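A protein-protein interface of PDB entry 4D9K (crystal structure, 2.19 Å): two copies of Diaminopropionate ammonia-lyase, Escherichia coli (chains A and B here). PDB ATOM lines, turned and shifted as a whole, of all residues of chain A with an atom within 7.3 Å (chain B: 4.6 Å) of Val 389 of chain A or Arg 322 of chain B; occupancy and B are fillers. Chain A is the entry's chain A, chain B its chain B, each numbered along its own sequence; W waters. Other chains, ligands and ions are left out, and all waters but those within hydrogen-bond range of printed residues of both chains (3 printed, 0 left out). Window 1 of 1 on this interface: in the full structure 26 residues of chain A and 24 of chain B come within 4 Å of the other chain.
ND2 of Asn 326 of chain A sits close to O of Gly 325 of chain B (3.4 Å).
The side-chain amide nitrogen (ND2) of Asn 326 of chain B lies within hydrogen-bond range of the side-chain hydroxyl (OH) of Tyr 385 of chain A (3.1 Å).
The backbone carbonyl oxygen (O) of Asn 326 of chain B sits at hydrogen-bond distance from the indole nitrogen (NE1) of Trp 390 of chain A, 2.6 Å away.
The backbone carbonyl oxygen of Trp 390 of chain A lies within hydrogen-bond range of the guanidinium group of Arg 322 of chain B, at 2.7 Å.
The guanidinium group of Arg 386 of chain A sits at hydrogen-bond distance from the backbone carbonyl oxygen of Asn 326 of chain B.
O of Gly 325 of chain A lies close to OD1 of Asn 326 of chain B (3.3 Å).
The side-chain amide oxygen (OD1) of Asn 326 of chain B lies within hydrogen-bond range of the guanidinium group (NH2) of Arg 333 of chain A (2.8 Å).
Of the 15 printed residues of chain B, 8 touch a printed residue of chain A.
Hydrophobic or aromatic side chains of chain B within 4 Å of the printed part of chain A: Leu 319, Val 323, Val 389 and Ala 395.
Of the 23 printed residues of chain A, 11 touch a printed residue of chain B.
Printed residues of chain A that touch a printed residue of chain B: Arg 322, Gly 325, Asn 326, Arg 333, Tyr 385, Arg 386, Val 389, Trp 390, Glu 391, Gly 392 and Ala 395.
Hydrophobic or aromatic side chains of chain A that line the printed part of chain B: Tyr 385, Val 389, Trp 390 and Ala 395.
Along chain A the printed residues that touch a printed residue of chain B span positions 322 to 395.
Among the printed residues, no Asp or Glu carboxylate lies within 4 Å of a Lys or Arg side-chain nitrogen of the other chain.
Water W2 bridges the backbone carbonyl oxygen (O) of Val 389 of chain A (2.6 Å) and the backbone carbonyl oxygen (O) of Val 389 of chain B (2.6 Å).
Water W1 lies within hydrogen-bond range of the side-chain amide nitrogen of Asn 326 of chain A, the backbone carbonyl oxygen of Arg 322 of chain B and the backbone NH of Asn 326 of chain B.
Printed residues of chain B within 4 Å of Asn 326 of chain A: Gly 325 (3.2 Å) and Val 389 (3.5 Å).
Ile 335 of chain A touches none of the printed residues of chain B.
Val 389 of chain A touches just these residues of chain B: Arg 322 and Asn 326.
Printed residues of chain B within 4 Å of Glu 391 of chain A: Arg 322 and Ala 395.
Arg 322 of chain B touches three residues of chain A.
Printed residues of chain A within 4 Å of Asn 326 of chain B: Gly 325, Arg 333, Tyr 385, Arg 386, Val 389 and Trp 390.
The nearest printed residue of chain B that does not touch Val 389 of chain A is Val 389 of chain B (4.9 Å).
The nearest residue of chain A that does not touch Arg 322 of chain B is Gly 392 of chain A (4.3 Å).
The nearest printed residue of chain B that does not touch Trp 390 of chain A is Ala 318 of chain B (5.1 Å).
Asn 326 of chain A touches Val 389 of chain B, and with the chains exchanged Val 389 of chain A touches Asn 326 of chain B.
Gly 392 of chain A touches Ala 395 of chain B, and with the chains exchanged Ala 395 of chain A touches Gly 392 of chain B.
12 positions are printed for both chains.
Of the 18 pairs that touch across the chains among the printed residues, 9 have their exchanged pair printed and touching as well.
NH2 of Arg 322 of chain B is in hydrogen-bond range of O of His 394 of chain B.
The guanidinium group of Arg 322 of chain B sits at hydrogen-bond distance from the backbone carbonyl oxygen of Val 388 of chain B, 3.0 Å away.
O of Gly 325 of chain A is in hydrogen-bond range of NE of Arg 333 of chain A.
Among the printed residues, merely in contact across the chains: Arg 322 of chain A with Val 389 of chain B (3.2 Å), Trp 390 of chain A with Val 323 of chain B (3.3 Å), Val 389 of chain A with Arg 322 of chain B (3.5 Å), Gly 392 of chain A with Ala 395 of chain B (3.5 Å), Val 389 of chain A with Asn 326 of chain B (3.5 Å), Ala 395 of chain A with Gly 392 of chain B (3.5 Å), Asn 326 of chain A with Val 389 of chain B (3.5 Å), Glu 391 of chain A with Ala 395 of chain B (3.5 Å), Trp 390 of chain A with Leu 319 of chain B (3.7 Å), Gly 325 of chain A with Gly 325 of chain B (3.8 Å) and Glu 391 of chain A with Arg 322 of chain B (3.9 Å).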
ATOM      1  N   ALA A 318      -0.418  21.216 -20.228  1.00  0.00           N
ATOM      2  CA  ALA A 318      -1.691  21.228 -20.953  1.00  0.00           C
ATOM      3  C   ALA A 318      -2.434  19.894 -20.841  1.00  0.00           C
ATOM      4  O   ALA A 318      -3.636  19.869 -20.577  1.00  0.00           O
ATOM      5  CB  ALA A 318      -1.461  21.573 -22.416  1.00  0.00           C
ATOM      6  N   GLY A 320      -2.049  17.614 -18.509  1.00  0.00           N
ATOM      7  CA  GLY A 320      -2.459  17.496 -17.114  1.00  0.00           C
ATOM      8  C   GLY A 320      -3.708  18.289 -16.783  1.00  0.00           C
ATOM      9  O   GLY A 320      -4.542  17.840 -15.993  1.00  0.00           O
ATOM     10  N   MET A 321      -3.829  19.467 -17.391  1.00  0.00           N
ATOM     11  CA  MET A 321      -5.002  20.316 -17.229  1.00  0.00           C
ATOM     12  C   MET A 321      -6.273  19.594 -17.677  1.00  0.00           C
ATOM     13  O   MET A 321      -7.288  19.597 -16.965  1.00  0.00           O
ATOM     14  CB  MET A 321      -4.826  21.637 -17.994  1.00  0.00           C
ATOM     15  CG  MET A 321      -3.724  22.519 -17.439  1.00  0.00           C
ATOM     16  SD  MET A 321      -3.168  23.849 -18.528  1.00  0.00           S
ATOM     17  CE  MET A 321      -4.473  25.063 -18.321  1.00  0.00           C
ATOM     18  N   ARG A 322      -6.195  18.957 -18.844  1.00  0.00           N
ATOM     19  CA  ARG A 322      -7.333  18.253 -19.427  1.00  0.00           C
ATOM     20  C   ARG A 322      -7.721  16.999 -18.638  1.00  0.00           C
ATOM     21  O   ARG A 322      -8.909  16.715 -18.455  1.00  0.00           O
ATOM     22  CB  ARG A 322      -7.055  17.894 -20.895  1.00  0.00           C
ATOM     23  CG  ARG A 322      -6.850  19.099 -21.801  1.00  0.00           C
ATOM     24  CD  ARG A 322      -6.714  18.713 -23.267  1.00  0.00           C
ATOM     25  NE  ARG A 322      -5.999  19.751 -24.012  1.00  0.00           N
ATOM     26  CZ  ARG A 322      -4.725  19.667 -24.379  1.00  0.00           C
ATOM     27  NH1 ARG A 322      -4.009  18.585 -24.099  1.00  0.00           N
ATOM     28  NH2 ARG A 322      -4.164  20.665 -25.036  1.00  0.00           N
ATOM     29  N   VAL A 323      -6.729  16.253 -18.169  1.00  0.00           N
ATOM     30  CA  VAL A 323      -7.011  15.036 -17.417  1.00  0.00           C
ATOM     31  C   VAL A 323      -7.687  15.402 -16.098  1.00  0.00           C
ATOM     32  O   VAL A 323      -8.662  14.771 -15.695  1.00  0.00           O
ATOM     33  CB  VAL A 323      -5.745  14.183 -17.176  1.00  0.00           C
ATOM     34  CG1 VAL A 323      -6.073  12.974 -16.316  1.00  0.00           C
ATOM     35  CG2 VAL A 323      -5.143  13.727 -18.503  1.00  0.00           C
ATOM     36  N   GLY A 325      -9.362  18.249 -15.452  1.00  0.00           N
ATOM     37  CA  GLY A 325     -10.617  18.958 -15.717  1.00  0.00           C
ATOM     38  C   GLY A 325     -11.737  18.160 -16.359  1.00  0.00           C
ATOM     39  O   GLY A 325     -12.904  18.542 -16.270  1.00  0.00           O
ATOM     40  N   ASN A 326     -11.390  17.065 -17.029  1.00  0.00           N
ATOM     41  CA  ASN A 326     -12.379  16.092 -17.474  1.00  0.00           C
ATOM     42  C   ASN A 326     -11.962  14.698 -16.968  1.00  0.00           C
ATOM     43  O   ASN A 326     -11.402  13.901 -17.720  1.00  0.00           O
ATOM     44  CB  ASN A 326     -12.537  16.122 -19.003  1.00  0.00           C
ATOM     45  CG  ASN A 326     -13.683  15.250 -19.500  1.00  0.00           C
ATOM     46  OD1 ASN A 326     -14.185  14.363 -18.785  1.00  0.00           O
ATOM     47  ND2 ASN A 326     -14.104  15.491 -20.732  1.00  0.00           N
ATOM     48  N   ARG A 333     -13.575  15.994 -10.255  1.00  0.00           N
ATOM     49  CA  ARG A 333     -13.031  16.941 -11.227  1.00  0.00           C
ATOM     50  C   ARG A 333     -12.286  18.069 -10.517  1.00  0.00           C
ATOM     51  O   ARG A 333     -12.742  18.567  -9.478  1.00  0.00           O
ATOM     52  CB  ARG A 333     -14.180  17.499 -12.075  1.00  0.00           C
ATOM     53  CG  ARG A 333     -13.821  18.623 -13.035  1.00  0.00           C
ATOM     54  CD  ARG A 333     -14.968  18.894 -13.997  1.00  0.00           C
ATOM     55  NE  ARG A 333     -14.840  20.215 -14.619  1.00  0.00           N
ATOM     56  CZ  ARG A 333     -15.608  21.258 -14.321  1.00  0.00           C
ATOM     57  NH1 ARG A 333     -16.587  21.134 -13.431  1.00  0.00           N
ATOM     58  NH2 ARG A 333     -15.410  22.418 -14.925  1.00  0.00           N
ATOM     59  N   ILE A 335     -10.022  21.795 -11.270  1.00  0.00           N
ATOM     60  CA  ILE A 335      -9.665  22.875 -12.193  1.00  0.00           C
ATOM     61  C   ILE A 335      -8.254  23.311 -11.865  1.00  0.00           C
ATOM     62  O   ILE A 335      -8.004  23.886 -10.807  1.00  0.00           O
ATOM     63  CB  ILE A 335     -10.618  24.075 -12.089  1.00  0.00           C
ATOM     64  CG1 ILE A 335     -12.075  23.634 -12.252  1.00  0.00           C
ATOM     65  CG2 ILE A 335     -10.240  25.156 -13.107  1.00  0.00           C
ATOM     66  CD1 ILE A 335     -13.040  24.802 -12.149  1.00  0.00           C
ATOM     67  N   SER A 336      -7.336  23.005 -12.775  1.00  0.00           N
ATOM     68  CA  SER A 336      -5.916  23.201 -12.553  1.00  0.00           C
ATOM     69  C   SER A 336      -5.311  24.023 -13.685  1.00  0.00           C
ATOM     70  O   SER A 336      -5.444  23.663 -14.856  1.00  0.00           O
ATOM     71  CB  SER A 336      -5.235  21.834 -12.473  1.00  0.00           C
ATOM     72  OG  SER A 336      -3.930  21.923 -11.934  1.00  0.00           O
ATOM     73  N   VAL A 382      -8.334  32.386 -17.133  1.00  0.00           N
ATOM     74  CA  VAL A 382      -9.515  31.718 -17.672  1.00  0.00           C
ATOM     75  C   VAL A 382      -9.427  31.530 -19.183  1.00  0.00           C
ATOM     76  O   VAL A 382      -9.787  30.468 -19.711  1.00  0.00           O
ATOM     77  CB  VAL A 382     -10.791  32.495 -17.255  1.00  0.00           C
ATOM     78  CG1 VAL A 382     -11.966  32.208 -18.174  1.00  0.00           C
ATOM     79  CG2 VAL A 382     -11.147  32.160 -15.813  1.00  0.00           C
ATOM     80  N   LYS A 383      -8.932  32.563 -19.867  1.00  0.00           N
ATOM     81  CA  LYS A 383      -8.753  32.536 -21.306  1.00  0.00           C
ATOM     82  C   LYS A 383      -7.837  31.384 -21.713  1.00  0.00           C
ATOM     83  O   LYS A 383      -8.217  30.540 -22.520  1.00  0.00           O
ATOM     84  CB  LYS A 383      -8.203  33.880 -21.789  1.00  0.00           C
ATOM     85  CG  LYS A 383      -7.816  33.908 -23.254  1.00  0.00           C
ATOM     86  CD  LYS A 383      -7.587  35.330 -23.755  1.00  0.00           C
ATOM     87  CE  LYS A 383      -7.237  35.328 -25.233  1.00  0.00           C
ATOM     88  NZ  LYS A 383      -6.068  34.443 -25.521  1.00  0.00           N
ATOM     89  N   HIS A 384      -6.636  31.352 -21.143  1.00  0.00           N
ATOM     90  CA  HIS A 384      -5.686  30.273 -21.392  1.00  0.00           C
ATOM     91  C   HIS A 384      -6.241  28.917 -20.969  1.00  0.00           C
ATOM     92  O   HIS A 384      -6.130  27.940 -21.715  1.00  0.00           O
ATOM     93  CB  HIS A 384      -4.356  30.591 -20.709  1.00  0.00           C
ATOM     94  CG  HIS A 384      -3.339  29.488 -20.810  1.00  0.00           C
ATOM     95  ND1 HIS A 384      -2.522  29.356 -21.864  1.00  0.00           N
ATOM     96  CD2 HIS A 384      -3.041  28.433 -19.941  1.00  0.00           C
ATOM     97  CE1 HIS A 384      -1.732  28.278 -21.689  1.00  0.00           C
ATOM     98  NE2 HIS A 384      -2.053  27.712 -20.511  1.00  0.00           N
ATOM     99  N   TYR A 385      -6.875  28.852 -19.801  1.00  0.00           N
ATOM    100  CA  TYR A 385      -7.452  27.582 -19.319  1.00  0.00           C
ATOM    101  C   TYR A 385      -8.435  26.962 -20.326  1.00  0.00           C
ATOM    102  O   TYR A 385      -8.321  25.782 -20.667  1.00  0.00           O
ATOM    103  CB  TYR A 385      -8.117  27.739 -17.945  1.00  0.00           C
ATOM    104  CG  TYR A 385      -8.653  26.426 -17.400  1.00  0.00           C
ATOM    105  CD1 TYR A 385      -7.811  25.528 -16.748  1.00  0.00           C
ATOM    106  CD2 TYR A 385      -9.992  26.068 -17.570  1.00  0.00           C
ATOM    107  CE1 TYR A 385      -8.293  24.310 -16.258  1.00  0.00           C
ATOM    108  CE2 TYR A 385     -10.482  24.859 -17.095  1.00  0.00           C
ATOM    109  CZ  TYR A 385      -9.632  23.987 -16.441  1.00  0.00           C
ATOM    110  OH  TYR A 385     -10.111  22.796 -15.976  1.00  0.00           O
ATOM    111  N   ARG A 386      -9.384  27.764 -20.811  1.00  0.00           N
ATOM    112  CA  ARG A 386     -10.393  27.280 -21.761  1.00  0.00           C
ATOM    113  C   ARG A 386      -9.846  27.087 -23.174  1.00  0.00           C
ATOM    114  O   ARG A 386     -10.448  26.390 -23.987  1.00  0.00           O
ATOM    115  CB  ARG A 386     -11.631  28.191 -21.772  1.00  0.00           C
ATOM    116  CG  ARG A 386     -12.345  28.278 -20.431  1.00  0.00           C
ATOM    117  CD  ARG A 386     -12.984  26.956 -20.030  1.00  0.00           C
ATOM    118  NE  ARG A 386     -13.374  26.953 -18.622  1.00  0.00           N
ATOM    119  CZ  ARG A 386     -14.004  25.952 -18.013  1.00  0.00           C
ATOM    120  NH1 ARG A 386     -14.328  24.857 -18.686  1.00  0.00           N
ATOM    121  NH2 ARG A 386     -14.309  26.049 -16.723  1.00  0.00           N
ATOM    122  N   GLU A 387      -8.717  27.724 -23.474  1.00  0.00           N
ATOM    123  CA  GLU A 387      -8.033  27.480 -24.737  1.00  0.00           C
ATOM    124  C   GLU A 387      -7.432  26.067 -24.696  1.00  0.00           C
ATOM    125  O   GLU A 387      -7.606  25.272 -25.620  1.00  0.00           O
ATOM    126  CB  GLU A 387      -6.975  28.551 -24.997  1.00  0.00           C
ATOM    127  CG  GLU A 387      -7.537  29.784 -25.694  1.00  0.00           C
ATOM    128  CD  GLU A 387      -6.680  31.031 -25.559  1.00  0.00           C
ATOM    129  OE1 GLU A 387      -5.491  30.949 -25.174  1.00  0.00           O
ATOM    130  OE2 GLU A 387      -7.208  32.118 -25.857  1.00  0.00           O
ATOM    131  N   VAL A 388      -6.756  25.757 -23.598  1.00  0.00           N
ATOM    132  CA  VAL A 388      -6.227  24.417 -23.375  1.00  0.00           C
ATOM    133  C   VAL A 388      -7.340  23.368 -23.355  1.00  0.00           C
ATOM    134  O   VAL A 388      -7.371  22.487 -24.208  1.00  0.00           O
ATOM    135  CB  VAL A 388      -5.380  24.345 -22.082  1.00  0.00           C
ATOM    136  CG1 VAL A 388      -4.955  22.910 -21.780  1.00  0.00           C
ATOM    137  CG2 VAL A 388      -4.159  25.244 -22.203  1.00  0.00           C
ATOM    138  N   VAL A 389      -8.261  23.485 -22.400  1.00  0.00           N
ATOM    139  CA  VAL A 389      -9.235  22.413 -22.141  1.00  0.00           C
ATOM    140  C   VAL A 389     -10.378  22.337 -23.161  1.00  0.00           C
ATOM    141  O   VAL A 389     -10.950  21.265 -23.354  1.00  0.00           O
ATOM    142  CB  VAL A 389      -9.790  22.426 -20.687  1.00  0.00           C
ATOM    143  CG1 VAL A 389      -8.669  22.603 -19.671  1.00  0.00           C
ATOM    144  CG2 VAL A 389     -10.875  23.477 -20.493  1.00  0.00           C
ATOM    145  N   TRP A 390     -10.699  23.453 -23.834  1.00  0.00           N
ATOM    146  CA  TRP A 390     -11.789  23.417 -24.819  1.00  0.00           C
ATOM    147  C   TRP A 390     -11.323  23.424 -26.234  1.00  0.00           C
ATOM    148  O   TRP A 390     -11.712  22.552 -27.019  1.00  0.00           O
ATOM    149  CB  TRP A 390     -12.797  24.547 -24.621  1.00  0.00           C
ATOM    150  CG  TRP A 390     -13.722  24.385 -23.450  1.00  0.00           C
ATOM    151  CD1 TRP A 390     -13.858  23.272 -22.607  1.00  0.00           C
ATOM    152  CD2 TRP A 390     -14.714  25.351 -22.964  1.00  0.00           C
ATOM    153  NE1 TRP A 390     -14.814  23.497 -21.656  1.00  0.00           N
ATOM    154  CE2 TRP A 390     -15.379  24.714 -21.816  1.00  0.00           C
ATOM    155  CE3 TRP A 390     -15.114  26.617 -23.354  1.00  0.00           C
ATOM    156  CZ2 TRP A 390     -16.386  25.351 -21.105  1.00  0.00           C
ATOM    157  CZ3 TRP A 390     -16.127  27.254 -22.623  1.00  0.00           C
ATOM    158  CH2 TRP A 390     -16.744  26.639 -21.533  1.00  0.00           C
ATOM    159  N   GLU A 391     -10.518  24.434 -26.581  1.00  0.00           N
ATOM    160  CA  GLU A 391     -10.018  24.615 -27.947  1.00  0.00           C
ATOM    161  C   GLU A 391      -8.910  23.624 -28.304  1.00  0.00           C
ATOM    162  O   GLU A 391      -8.643  23.385 -29.471  1.00  0.00           O
ATOM    163  CB  GLU A 391      -9.511  26.048 -28.159  1.00  0.00           C
ATOM    164  CG  GLU A 391     -10.487  27.161 -27.794  1.00  0.00           C
ATOM    165  CD  GLU A 391      -9.932  28.543 -28.133  1.00  0.00           C
ATOM    166  OE1 GLU A 391      -8.842  28.609 -28.737  1.00  0.00           O
ATOM    167  OE2 GLU A 391     -10.577  29.567 -27.796  1.00  0.00           O
ATOM    168  N   GLY A 392      -8.256  23.068 -27.295  1.00  0.00           N
ATOM    169  CA  GLY A 392      -7.254  22.031 -27.514  1.00  0.00           C
ATOM    170  C   GLY A 392      -5.871  22.591 -27.767  1.00  0.00           C
ATOM    171  O   GLY A 392      -5.058  21.949 -28.435  1.00  0.00           O
ATOM    172  N   LYS A 393      -5.605  23.786 -27.235  1.00  0.00           N
ATOM    173  CA  LYS A 393      -4.289  24.429 -27.363  1.00  0.00           C
ATOM    174  C   LYS A 393      -3.208  23.575 -26.700  1.00  0.00           C
ATOM    175  O   LYS A 393      -3.455  22.955 -25.664  1.00  0.00           O
ATOM    176  CB  LYS A 393      -4.300  25.834 -26.750  1.00  0.00           C
ATOM    177  CG  LYS A 393      -3.103  26.694 -27.135  1.00  0.00           C
ATOM    178  CD  LYS A 393      -3.277  28.147 -26.717  1.00  0.00           C
ATOM    179  CE  LYS A 393      -2.721  28.418 -25.324  1.00  0.00           C
ATOM    180  NZ  LYS A 393      -3.000  29.809 -24.865  1.00  0.00           N
ATOM    181  N   ALA A 395      -1.912  20.819 -27.981  1.00  0.00           N
ATOM    182  CA  ALA A 395      -2.351  19.441 -28.153  1.00  0.00           C
ATOM    183  C   ALA A 395      -1.161  18.498 -28.263  1.00  0.00           C
ATOM    184  O   ALA A 395      -0.057  18.915 -28.626  1.00  0.00           O
ATOM    185  CB  ALA A 395      -3.239  19.311 -29.382  1.00  0.00           C
ATOM    186  N   ALA B 318     -15.740  18.092 -31.994  1.00  0.00           N
ATOM    187  CA  ALA B 318     -14.653  17.922 -31.034  1.00  0.00           C
ATOM    188  C   ALA B 318     -14.724  18.991 -29.949  1.00  0.00           C
ATOM    189  O   ALA B 318     -14.578  18.696 -28.757  1.00  0.00           O
ATOM    190  CB  ALA B 318     -13.303  17.952 -31.738  1.00  0.00           C
ATOM    191  N   LEU B 319     -14.963  20.230 -30.376  1.00  0.00           N
ATOM    192  CA  LEU B 319     -15.177  21.348 -29.469  1.00  0.00           C
ATOM    193  C   LEU B 319     -16.345  21.108 -28.496  1.00  0.00           C
ATOM    194  O   LEU B 319     -16.229  21.386 -27.302  1.00  0.00           O
ATOM    195  CB  LEU B 319     -15.402  22.636 -30.274  1.00  0.00           C
ATOM    196  CG  LEU B 319     -15.691  23.924 -29.512  1.00  0.00           C
ATOM    197  CD1 LEU B 319     -14.538  24.262 -28.575  1.00  0.00           C
ATOM    198  CD2 LEU B 319     -15.962  25.067 -30.492  1.00  0.00           C
ATOM    199  N   GLY B 320     -17.460  20.598 -29.010  1.00  0.00           N
ATOM    200  CA  GLY B 320     -18.628  20.300 -28.182  1.00  0.00           C
ATOM    201  C   GLY B 320     -18.357  19.227 -27.142  1.00  0.00           C
ATOM    202  O   GLY B 320     -18.846  19.312 -26.022  1.00  0.00           O
ATOM    203  N   MET B 321     -17.569  18.224 -27.516  1.00  0.00           N
ATOM    204  CA  MET B 321     -17.215  17.143 -26.587  1.00  0.00           C
ATOM    205  C   MET B 321     -16.442  17.707 -25.396  1.00  0.00           C
ATOM    206  O   MET B 321     -16.688  17.322 -24.254  1.00  0.00           O
ATOM    207  CB  MET B 321     -16.385  16.073 -27.293  1.00  0.00           C
ATOM    208  CG  MET B 321     -17.111  15.341 -28.411  1.00  0.00           C
ATOM    209  SD  MET B 321     -15.976  14.316 -29.368  1.00  0.00           S
ATOM    210  CE  MET B 321     -15.807  12.882 -28.299  1.00  0.00           C
ATOM    211  N   ARG B 322     -15.536  18.644 -25.676  1.00  0.00           N
ATOM    212  CA  ARG B 322     -14.667  19.240 -24.661  1.00  0.00           C
ATOM    213  C   ARG B 322     -15.413  20.203 -23.748  1.00  0.00           C
ATOM    214  O   ARG B 322     -15.148  20.251 -22.551  1.00  0.00           O
ATOM    215  CB  ARG B 322     -13.484  19.972 -25.311  1.00  0.00           C
ATOM    216  CG  ARG B 322     -12.634  19.095 -26.210  1.00  0.00           C
ATOM    217  CD  ARG B 322     -11.245  19.657 -26.419  1.00  0.00           C
ATOM    218  NE  ARG B 322     -10.659  19.112 -27.640  1.00  0.00           N
ATOM    219  CZ  ARG B 322     -10.783  19.662 -28.843  1.00  0.00           C
ATOM    220  NH1 ARG B 322     -11.467  20.786 -29.004  1.00  0.00           N
ATOM    221  NH2 ARG B 322     -10.226  19.085 -29.888  1.00  0.00           N
ATOM    222  N   VAL B 323     -16.317  20.990 -24.330  1.00  0.00           N
ATOM    223  CA  VAL B 323     -17.082  21.992 -23.587  1.00  0.00           C
ATOM    224  C   VAL B 323     -18.060  21.301 -22.636  1.00  0.00           C
ATOM    225  O   VAL B 323     -18.197  21.704 -21.480  1.00  0.00           O
ATOM    226  CB  VAL B 323     -17.833  22.962 -24.528  1.00  0.00           C
ATOM    227  CG1 VAL B 323     -18.734  23.900 -23.733  1.00  0.00           C
ATOM    228  CG2 VAL B 323     -16.855  23.769 -25.379  1.00  0.00           C
ATOM    229  N   LEU B 324     -18.731  20.266 -23.131  1.00  0.00           N
ATOM    230  CA  LEU B 324     -19.654  19.480 -22.316  1.00  0.00           C
ATOM    231  C   LEU B 324     -18.952  18.680 -21.219  1.00  0.00           C
ATOM    232  O   LEU B 324     -19.495  18.526 -20.128  1.00  0.00           O
ATOM    233  CB  LEU B 324     -20.480  18.528 -23.188  1.00  0.00           C
ATOM    234  CG  LEU B 324     -21.693  19.071 -23.940  1.00  0.00           C
ATOM    235  CD1 LEU B 324     -22.156  18.056 -24.971  1.00  0.00           C
ATOM    236  CD2 LEU B 324     -22.843  19.457 -23.024  1.00  0.00           C
ATOM    237  N   GLY B 325     -17.757  18.175 -21.520  1.00  0.00           N
ATOM    238  CA  GLY B 325     -17.001  17.313 -20.601  1.00  0.00           C
ATOM    239  C   GLY B 325     -16.166  18.058 -19.575  1.00  0.00           C
ATOM    240  O   GLY B 325     -15.774  17.490 -18.558  1.00  0.00           O
ATOM    241  N   ASN B 326     -15.869  19.326 -19.854  1.00  0.00           N
ATOM    242  CA  ASN B 326     -15.291  20.212 -18.846  1.00  0.00           C
ATOM    243  C   ASN B 326     -16.111  21.494 -18.826  1.00  0.00           C
ATOM    244  O   ASN B 326     -15.774  22.462 -19.531  1.00  0.00           O
ATOM    245  CB  ASN B 326     -13.810  20.492 -19.124  1.00  0.00           C
ATOM    246  CG  ASN B 326     -13.105  21.166 -17.955  1.00  0.00           C
ATOM    247  OD1 ASN B 326     -13.739  21.636 -17.006  1.00  0.00           O
ATOM    248  ND2 ASN B 326     -11.778  21.205 -18.013  1.00  0.00           N
ATOM    249  N   VAL B 388      -9.799  13.182 -27.875  1.00  0.00           N
ATOM    250  CA  VAL B 388     -10.384  14.514 -28.037  1.00  0.00           C
ATOM    251  C   VAL B 388     -10.223  15.337 -26.755  1.00  0.00           C
ATOM    252  O   VAL B 388      -9.662  16.433 -26.784  1.00  0.00           O
ATOM    253  CB  VAL B 388     -11.872  14.454 -28.472  1.00  0.00           C
ATOM    254  CG1 VAL B 388     -12.486  15.851 -28.521  1.00  0.00           C
ATOM    255  CG2 VAL B 388     -12.006  13.781 -29.831  1.00  0.00           C
ATOM    256  N   VAL B 389     -10.690  14.793 -25.631  1.00  0.00           N
ATOM    257  CA  VAL B 389     -10.767  15.577 -24.395  1.00  0.00           C
ATOM    258  C   VAL B 389      -9.448  15.726 -23.626  1.00  0.00           C
ATOM    259  O   VAL B 389      -9.270  16.701 -22.903  1.00  0.00           O
ATOM    260  CB  VAL B 389     -11.936  15.135 -23.474  1.00  0.00           C
ATOM    261  CG1 VAL B 389     -13.234  15.081 -24.266  1.00  0.00           C
ATOM    262  CG2 VAL B 389     -11.655  13.798 -22.790  1.00  0.00           C
ATOM    263  N   GLY B 392      -6.343  16.487 -27.030  1.00  0.00           N
ATOM    264  CA  GLY B 392      -6.711  17.625 -27.841  1.00  0.00           C
ATOM    265  C   GLY B 392      -6.740  17.310 -29.322  1.00  0.00           C
ATOM    266  O   GLY B 392      -6.449  18.185 -30.141  1.00  0.00           O
ATOM    267  N   LYS B 393      -7.080  16.065 -29.666  1.00  0.00           N
ATOM    268  CA  LYS B 393      -7.252  15.662 -31.071  1.00  0.00           C
ATOM    269  C   LYS B 393      -8.368  16.488 -31.701  1.00  0.00           C
ATOM    270  O   LYS B 393      -9.372  16.782 -31.048  1.00  0.00           O
ATOM    271  CB  LYS B 393      -7.565  14.163 -31.199  1.00  0.00           C
ATOM    272  CG  LYS B 393      -7.608  13.644 -32.636  1.00  0.00           C
ATOM    273  CD  LYS B 393      -7.743  12.124 -32.724  1.00  0.00           C
ATOM    274  CE  LYS B 393      -9.180  11.659 -32.527  1.00  0.00           C
ATOM    275  NZ  LYS B 393      -9.288  10.170 -32.473  1.00  0.00           N
ATOM    276  N   HIS B 394      -8.180  16.844 -32.973  1.00  0.00           N
ATOM    277  CA  HIS B 394      -9.066  17.769 -33.685  1.00  0.00           C
ATOM    278  C   HIS B 394      -9.178  19.057 -32.929  1.00  0.00           C
ATOM    279  O   HIS B 394     -10.274  19.541 -32.649  1.00  0.00           O
ATOM    280  CB  HIS B 394     -10.443  17.156 -33.949  1.00  0.00           C
ATOM    281  CG  HIS B 394     -10.395  15.868 -34.738  1.00  0.00           C
ATOM    282  ND1 HIS B 394     -10.974  14.730 -34.303  1.00  0.00           N
ATOM    283  CD2 HIS B 394      -9.802  15.566 -35.960  1.00  0.00           C
ATOM    284  CE1 HIS B 394     -10.768  13.751 -35.202  1.00  0.00           C
ATOM    285  NE2 HIS B 394     -10.047  14.263 -36.214  1.00  0.00           N
ATOM    286  N   ALA B 395      -8.023  19.609 -32.572  1.00  0.00           N
ATOM    287  CA  ALA B 395      -7.948  20.885 -31.878  1.00  0.00           C
ATOM    288  C   ALA B 395      -8.508  21.994 -32.770  1.00  0.00           C
ATOM    289  O   ALA B 395      -8.551  21.853 -33.994  1.00  0.00           O
ATOM    290  CB  ALA B 395      -6.510  21.185 -31.480  1.00  0.00           C
HETATM  291  O   HOH W   1     -13.675  17.869 -21.721  1.00  0.00           O
HETATM  292  O   HOH W   2     -10.742  18.829 -22.572  1.00  0.00           O
HETATM  293  O   HOH W   3     -10.499  18.775 -19.178  1.00  0.00           O
